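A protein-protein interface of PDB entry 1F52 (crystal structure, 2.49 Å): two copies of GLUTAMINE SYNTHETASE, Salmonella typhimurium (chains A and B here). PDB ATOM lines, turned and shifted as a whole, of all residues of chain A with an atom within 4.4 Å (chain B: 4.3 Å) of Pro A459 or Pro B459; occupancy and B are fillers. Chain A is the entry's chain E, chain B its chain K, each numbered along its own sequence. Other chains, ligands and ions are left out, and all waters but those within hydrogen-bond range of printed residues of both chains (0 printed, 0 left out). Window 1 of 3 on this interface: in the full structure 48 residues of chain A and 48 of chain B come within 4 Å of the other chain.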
ATOM      1  N   GLY A 141      -0.689  20.510  17.128  1.00  0.00           N
ATOM      2  CA  GLY A 141      -0.970  21.105  15.844  1.00  0.00           C
ATOM      3  C   GLY A 141      -2.370  20.748  15.399  1.00  0.00           C
ATOM      4  O   GLY A 141      -3.034  19.902  16.003  1.00  0.00           O
ATOM      5  N   SER A 147      -5.231  16.638  13.744  1.00  0.00           N
ATOM      6  CA  SER A 147      -4.765  17.457  14.861  1.00  0.00           C
ATOM      7  C   SER A 147      -4.211  16.548  15.933  1.00  0.00           C
ATOM      8  O   SER A 147      -4.491  15.343  15.950  1.00  0.00           O
ATOM      9  CB  SER A 147      -5.881  18.305  15.447  1.00  0.00           C
ATOM     10  OG  SER A 147      -6.943  17.498  15.929  1.00  0.00           O
ATOM     11  N   HIS A 148      -3.437  17.115  16.838  1.00  0.00           N
ATOM     12  CA  HIS A 148      -2.875  16.301  17.896  1.00  0.00           C
ATOM     13  C   HIS A 148      -2.231  17.112  18.980  1.00  0.00           C
ATOM     14  O   HIS A 148      -1.970  18.307  18.826  1.00  0.00           O
ATOM     15  CB  HIS A 148      -1.776  15.387  17.333  1.00  0.00           C
ATOM     16  CG  HIS A 148      -0.494  16.174  16.961  1.00  0.00           C
ATOM     17  ND1 HIS A 148      -0.391  16.927  15.809  1.00  0.00           N
ATOM     18  CD2 HIS A 148       0.691  16.315  17.607  1.00  0.00           C
ATOM     19  CE1 HIS A 148       0.800  17.503  15.766  1.00  0.00           C
ATOM     20  NE2 HIS A 148       1.472  17.146  16.845  1.00  0.00           N
ATOM     21  N   VAL A 149      -1.958  16.438  20.098  1.00  0.00           N
ATOM     22  CA  VAL A 149      -1.236  17.017  21.217  1.00  0.00           C
ATOM     23  C   VAL A 149      -0.527  15.883  21.898  1.00  0.00           C
ATOM     24  O   VAL A 149      -1.115  14.844  22.190  1.00  0.00           O
ATOM     25  CB  VAL A 149      -2.127  17.717  22.287  1.00  0.00           C
ATOM     26  CG1 VAL A 149      -3.215  16.784  22.771  1.00  0.00           C
ATOM     27  CG2 VAL A 149      -1.270  18.223  23.450  1.00  0.00           C
ATOM     28  N   PRO A 457     -12.782  19.195  14.521  1.00  0.00           N
ATOM     29  CA  PRO A 457     -13.020  17.811  14.938  1.00  0.00           C
ATOM     30  C   PRO A 457     -12.066  17.407  16.036  1.00  0.00           C
ATOM     31  O   PRO A 457     -10.903  17.786  16.021  1.00  0.00           O
ATOM     32  CB  PRO A 457     -12.752  17.028  13.669  1.00  0.00           C
ATOM     33  CG  PRO A 457     -13.281  17.957  12.605  1.00  0.00           C
ATOM     34  CD  PRO A 457     -12.739  19.309  13.052  1.00  0.00           C
ATOM     35  N   HIS A 458     -12.584  16.678  17.012  1.00  0.00           N
ATOM     36  CA  HIS A 458     -11.803  16.220  18.145  1.00  0.00           C
ATOM     37  C   HIS A 458     -11.365  14.778  17.936  1.00  0.00           C
ATOM     38  O   HIS A 458     -12.169  13.929  17.562  1.00  0.00           O
ATOM     39  CB  HIS A 458     -12.686  16.289  19.379  1.00  0.00           C
ATOM     40  CG  HIS A 458     -11.978  16.005  20.662  1.00  0.00           C
ATOM     41  ND1 HIS A 458     -12.048  16.846  21.746  1.00  0.00           N
ATOM     42  CD2 HIS A 458     -11.182  14.972  21.037  1.00  0.00           C
ATOM     43  CE1 HIS A 458     -11.329  16.352  22.737  1.00  0.00           C
ATOM     44  NE2 HIS A 458     -10.794  15.213  22.331  1.00  0.00           N
ATOM     45  N   PRO A 459     -10.109  14.457  18.250  1.00  0.00           N
ATOM     46  CA  PRO A 459      -9.596  13.096  18.089  1.00  0.00           C
ATOM     47  C   PRO A 459     -10.549  12.036  18.618  1.00  0.00           C
ATOM     48  O   PRO A 459     -10.795  11.032  17.953  1.00  0.00           O
ATOM     49  CB  PRO A 459      -8.320  13.126  18.908  1.00  0.00           C
ATOM     50  CG  PRO A 459      -7.801  14.522  18.600  1.00  0.00           C
ATOM     51  CD  PRO A 459      -9.044  15.369  18.723  1.00  0.00           C
ATOM     52  N   VAL A 460     -11.146  12.302  19.774  1.00  0.00           N
ATOM     53  CA  VAL A 460     -12.069  11.354  20.401  1.00  0.00           C
ATOM     54  C   VAL A 460     -13.322  11.108  19.562  1.00  0.00           C
ATOM     55  O   VAL A 460     -13.925  10.026  19.604  1.00  0.00           O
ATOM     56  CB  VAL A 460     -12.440  11.819  21.811  1.00  0.00           C
ATOM     57  CG1 VAL A 460     -13.481  10.926  22.411  1.00  0.00           C
ATOM     58  CG2 VAL A 460     -11.203  11.804  22.677  1.00  0.00           C
ATOM     59  N   GLU A 461     -13.673  12.081  18.733  1.00  0.00           N
ATOM     60  CA  GLU A 461     -14.841  11.923  17.890  1.00  0.00           C
ATOM     61  C   GLU A 461     -14.626  10.821  16.886  1.00  0.00           C
ATOM     62  O   GLU A 461     -15.581  10.194  16.441  1.00  0.00           O
ATOM     63  CB  GLU A 461     -15.186  13.229  17.192  1.00  0.00           C
ATOM     64  CG  GLU A 461     -15.776  14.235  18.176  1.00  0.00           C
ATOM     65  CD  GLU A 461     -16.081  15.585  17.569  1.00  0.00           C
ATOM     66  OE1 GLU A 461     -16.916  16.307  18.148  1.00  0.00           O
ATOM     67  OE2 GLU A 461     -15.468  15.946  16.547  1.00  0.00           O
ATOM     68  N   PHE A 462     -13.360  10.581  16.527  1.00  0.00           N
ATOM     69  CA  PHE A 462     -13.033   9.497  15.578  1.00  0.00           C
ATOM     70  C   PHE A 462     -13.183   8.146  16.260  1.00  0.00           C
ATOM     71  O   PHE A 462     -13.719   7.202  15.688  1.00  0.00           O
ATOM     72  CB  PHE A 462     -11.611   9.691  15.028  1.00  0.00           C
ATOM     73  CG  PHE A 462     -11.611  10.898  14.141  1.00  0.00           C
ATOM     74  CD1 PHE A 462     -11.781  10.779  12.779  1.00  0.00           C
ATOM     75  CD2 PHE A 462     -11.507  12.164  14.685  1.00  0.00           C
ATOM     76  CE1 PHE A 462     -11.860  11.905  11.967  1.00  0.00           C
ATOM     77  CE2 PHE A 462     -11.587  13.293  13.879  1.00  0.00           C
ATOM     78  CZ  PHE A 462     -11.766  13.157  12.521  1.00  0.00           C
ATOM     79  N   GLU A 463     -12.703   8.075  17.487  1.00  0.00           N
ATOM     80  CA  GLU A 463     -12.806   6.874  18.259  1.00  0.00           C
ATOM     81  C   GLU A 463     -14.271   6.510  18.407  1.00  0.00           C
ATOM     82  O   GLU A 463     -14.669   5.359  18.195  1.00  0.00           O
ATOM     83  CB  GLU A 463     -12.139   7.111  19.596  1.00  0.00           C
ATOM     84  CG  GLU A 463     -12.135   5.939  20.523  1.00  0.00           C
ATOM     85  CD  GLU A 463     -11.702   6.360  21.905  1.00  0.00           C
ATOM     86  OE1 GLU A 463     -10.803   7.221  22.030  1.00  0.00           O
ATOM     87  OE2 GLU A 463     -12.261   5.825  22.891  1.00  0.00           O
ATOM     88  N   GLY B 141      -6.119   8.248  18.424  1.00  0.00           N
ATOM     89  CA  GLY B 141      -5.932   7.699  19.745  1.00  0.00           C
ATOM     90  C   GLY B 141      -6.049   8.791  20.786  1.00  0.00           C
ATOM     91  O   GLY B 141      -6.096   9.978  20.459  1.00  0.00           O
ATOM     92  N   SER B 147      -3.515  13.059  22.564  1.00  0.00           N
ATOM     93  CA  SER B 147      -4.512  12.496  21.656  1.00  0.00           C
ATOM     94  C   SER B 147      -4.241  13.006  20.260  1.00  0.00           C
ATOM     95  O   SER B 147      -3.535  14.005  20.075  1.00  0.00           O
ATOM     96  CB  SER B 147      -5.927  12.871  22.063  1.00  0.00           C
ATOM     97  OG  SER B 147      -6.107  14.277  22.068  1.00  0.00           O
ATOM     98  N   HIS B 148      -4.807  12.336  19.273  1.00  0.00           N
ATOM     99  CA  HIS B 148      -4.589  12.772  17.910  1.00  0.00           C
ATOM    100  C   HIS B 148      -5.483  12.082  16.924  1.00  0.00           C
ATOM    101  O   HIS B 148      -6.112  11.066  17.223  1.00  0.00           O
ATOM    102  CB  HIS B 148      -3.149  12.461  17.476  1.00  0.00           C
ATOM    103  CG  HIS B 148      -2.921  10.944  17.257  1.00  0.00           C
ATOM    104  ND1 HIS B 148      -2.747  10.059  18.301  1.00  0.00           N
ATOM    105  CD2 HIS B 148      -2.860  10.201  16.123  1.00  0.00           C
ATOM    106  CE1 HIS B 148      -2.597   8.834  17.819  1.00  0.00           C
ATOM    107  NE2 HIS B 148      -2.663   8.898  16.501  1.00  0.00           N
ATOM    108  N   VAL B 149      -5.525  12.643  15.715  1.00  0.00           N
ATOM    109  CA  VAL B 149      -6.244  12.062  14.595  1.00  0.00           C
ATOM    110  C   VAL B 149      -5.526  12.505  13.354  1.00  0.00           C
ATOM    111  O   VAL B 149      -5.226  13.685  13.173  1.00  0.00           O
ATOM    112  CB  VAL B 149      -7.728  12.509  14.458  1.00  0.00           C
ATOM    113  CG1 VAL B 149      -7.834  14.018  14.439  1.00  0.00           C
ATOM    114  CG2 VAL B 149      -8.361  11.894  13.207  1.00  0.00           C
ATOM    115  N   PRO B 457      -9.073  16.836  26.927  1.00  0.00           N
ATOM    116  CA  PRO B 457      -8.450  18.035  26.359  1.00  0.00           C
ATOM    117  C   PRO B 457      -8.368  17.937  24.855  1.00  0.00           C
ATOM    118  O   PRO B 457      -8.109  16.871  24.312  1.00  0.00           O
ATOM    119  CB  PRO B 457      -7.067  18.021  26.980  1.00  0.00           C
ATOM    120  CG  PRO B 457      -7.346  17.484  28.360  1.00  0.00           C
ATOM    121  CD  PRO B 457      -8.301  16.331  28.077  1.00  0.00           C
ATOM    122  N   HIS B 458      -8.641  19.047  24.188  1.00  0.00           N
ATOM    123  CA  HIS B 458      -8.618  19.115  22.739  1.00  0.00           C
ATOM    124  C   HIS B 458      -7.302  19.711  22.259  1.00  0.00           C
ATOM    125  O   HIS B 458      -6.856  20.733  22.773  1.00  0.00           O
ATOM    126  CB  HIS B 458      -9.754  20.022  22.296  1.00  0.00           C
ATOM    127  CG  HIS B 458      -9.970  20.065  20.821  1.00  0.00           C
ATOM    128  ND1 HIS B 458     -11.201  19.852  20.247  1.00  0.00           N
ATOM    129  CD2 HIS B 458      -9.112  20.299  19.796  1.00  0.00           C
ATOM    130  CE1 HIS B 458     -11.099  19.948  18.933  1.00  0.00           C
ATOM    131  NE2 HIS B 458      -9.840  20.222  18.635  1.00  0.00           N
ATOM    132  N   PRO B 459      -6.702  19.134  21.218  1.00  0.00           N
ATOM    133  CA  PRO B 459      -5.438  19.636  20.680  1.00  0.00           C
ATOM    134  C   PRO B 459      -5.418  21.147  20.516  1.00  0.00           C
ATOM    135  O   PRO B 459      -4.453  21.804  20.898  1.00  0.00           O
ATOM    136  CB  PRO B 459      -5.357  18.950  19.331  1.00  0.00           C
ATOM    137  CG  PRO B 459      -5.925  17.579  19.659  1.00  0.00           C
ATOM    138  CD  PRO B 459      -7.135  17.916  20.496  1.00  0.00           C
ATOM    139  N   VAL B 460      -6.522  21.703  20.027  1.00  0.00           N
ATOM    140  CA  VAL B 460      -6.626  23.144  19.801  1.00  0.00           C
ATOM    141  C   VAL B 460      -6.532  23.952  21.095  1.00  0.00           C
ATOM    142  O   VAL B 460      -6.070  25.102  21.106  1.00  0.00           O
ATOM    143  CB  VAL B 460      -7.910  23.479  19.041  1.00  0.00           C
ATOM    144  CG1 VAL B 460      -8.087  24.961  18.918  1.00  0.00           C
ATOM    145  CG2 VAL B 460      -7.842  22.863  17.663  1.00  0.00           C
ATOM    146  N   GLU B 461      -6.896  23.325  22.205  1.00  0.00           N
ATOM    147  CA  GLU B 461      -6.825  24.015  23.477  1.00  0.00           C
ATOM    148  C   GLU B 461      -5.394  24.323  23.835  1.00  0.00           C
ATOM    149  O   GLU B 461      -5.129  25.282  24.551  1.00  0.00           O
ATOM    150  CB  GLU B 461      -7.492  23.198  24.573  1.00  0.00           C
ATOM    151  CG  GLU B 461      -9.009  23.210  24.417  1.00  0.00           C
ATOM    152  CD  GLU B 461      -9.741  22.361  25.431  1.00  0.00           C
ATOM    153  OE1 GLU B 461     -10.939  22.621  25.651  1.00  0.00           O
ATOM    154  OE2 GLU B 461      -9.142  21.416  25.979  1.00  0.00           O
ATOM    155  N   PHE B 462      -4.466  23.501  23.333  1.00  0.00           N
ATOM    156  CA  PHE B 462      -3.029  23.734  23.591  1.00  0.00           C
ATOM    157  C   PHE B 462      -2.541  24.921  22.774  1.00  0.00           C
ATOM    158  O   PHE B 462      -1.797  25.765  23.265  1.00  0.00           O
ATOM    159  CB  PHE B 462      -2.224  22.465  23.268  1.00  0.00           C
ATOM    160  CG  PHE B 462      -2.563  21.423  24.289  1.00  0.00           C
ATOM    161  CD1 PHE B 462      -1.785  21.250  25.412  1.00  0.00           C
ATOM    162  CD2 PHE B 462      -3.707  20.658  24.154  1.00  0.00           C
ATOM    163  CE1 PHE B 462      -2.144  20.336  26.397  1.00  0.00           C
ATOM    164  CE2 PHE B 462      -4.071  19.745  25.135  1.00  0.00           C
ATOM    165  CZ  PHE B 462      -3.288  19.590  26.257  1.00  0.00           C
ATOM    166  N   GLU B 463      -2.974  24.968  21.529  1.00  0.00           N
ATOM    167  CA  GLU B 463      -2.620  26.047  20.658  1.00  0.00           C
ATOM    168  C   GLU B 463      -3.097  27.349  21.270  1.00  0.00           C
ATOM    169  O   GLU B 463      -2.352  28.333  21.347  1.00  0.00           O
ATOM    170  CB  GLU B 463      -3.247  25.791  19.304  1.00  0.00           C
ATOM    171  CG  GLU B 463      -2.954  26.817  18.260  1.00  0.00           C
ATOM    172  CD  GLU B 463      -3.837  26.612  17.056  1.00  0.00           C
ATOM    173  OE1 GLU B 463      -4.111  25.448  16.686  1.00  0.00           O
ATOM    174  OE2 GLU B 463      -4.270  27.625  16.458  1.00  0.00           O
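Among the printed residues, pairs that only touch across the chains: Ser A147 with His B148, Ser A147 with Pro B459, His A148 with Ser B147, His A148 with His B148, His A148 with Pro B459, Val A149 with Phe B462, Pro A457 with His B458, His A458 with Pro B457, Pro A459 with Ser B147, Pro A459 with His B148, Pro A459 with Pro B459 and Phe A462 with Val B149.
Printed residues of chain B that touch a printed residue of chain A: Ser B147, His B148, Val B149, Pro B457, His B458, Pro B459 and Phe B462.
Among the printed residues, 15 pairs touch across the chains.
The backbone carbonyl oxygen (O) of Gly A141 is in hydrogen-bond range of the backbone NH (N) of His A148, 2.9 Å away.
N of His A458 lies within hydrogen-bond range of OE2 of Glu A461 (3.0 Å).
O of Gly B141 sits at hydrogen-bond distance from N of His B148, 2.9 Å away.
OE2 of Glu B461 lies within hydrogen-bond range of N of His B458, 3.0 Å away.
The backbone NH (N) of Val B149 sits at hydrogen-bond distance from the backbone carbonyl oxygen (O) of Ser A147.
The backbone carbonyl oxygen of Ser B147 is in hydrogen-bond range of the backbone NH of Val A149 (2.9 Å).
A ring nitrogen (ND1) of His B458 sits at hydrogen-bond distance from a ring nitrogen (ND1) of His A458 (3.5 Å).
Printed residues of chain B within 4 Å of His A458: Pro B457 (3.6 Å) and His B458 (3.5 Å).
Printed residues of chain B within 4 Å of Pro A459: Ser B147 (3.9 Å), His B148 (3.5 Å) and Pro B459 (3.6 Å).
Of the printed residues of chain B, Phe A462 touches Val B149.
Of the printed residues of chain A, His B458 touches Pro A457 (3.6 Å) and His A458 (3.5 Å).
Of chain A, only Ser A147 (3.9 Å), His A148 (3.5 Å) and Pro A459 (3.6 Å) come within 4 Å of Pro B459.
Val B460 touches none of the printed residues of chain A.
Glu B463 touches none of the printed residues of chain A.
The nearest printed residue of chain A that does not touch Pro B459 is Val A149 (4.2 Å).
Ser A147 touches Pro B459, and with the chains exchanged Pro A459 touches Ser B147.
His A148 touches Pro B459, and with the chains exchanged Pro A459 touches His B148.
Pro A457 touches His B458, and with the chains exchanged His A458 touches Pro B457.
His A458 touches its own counterpart, His B458.
Positions printed for both chains: 141, 147, 148, 149, 457, 458, 459, 460, 461, 462 and 463.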
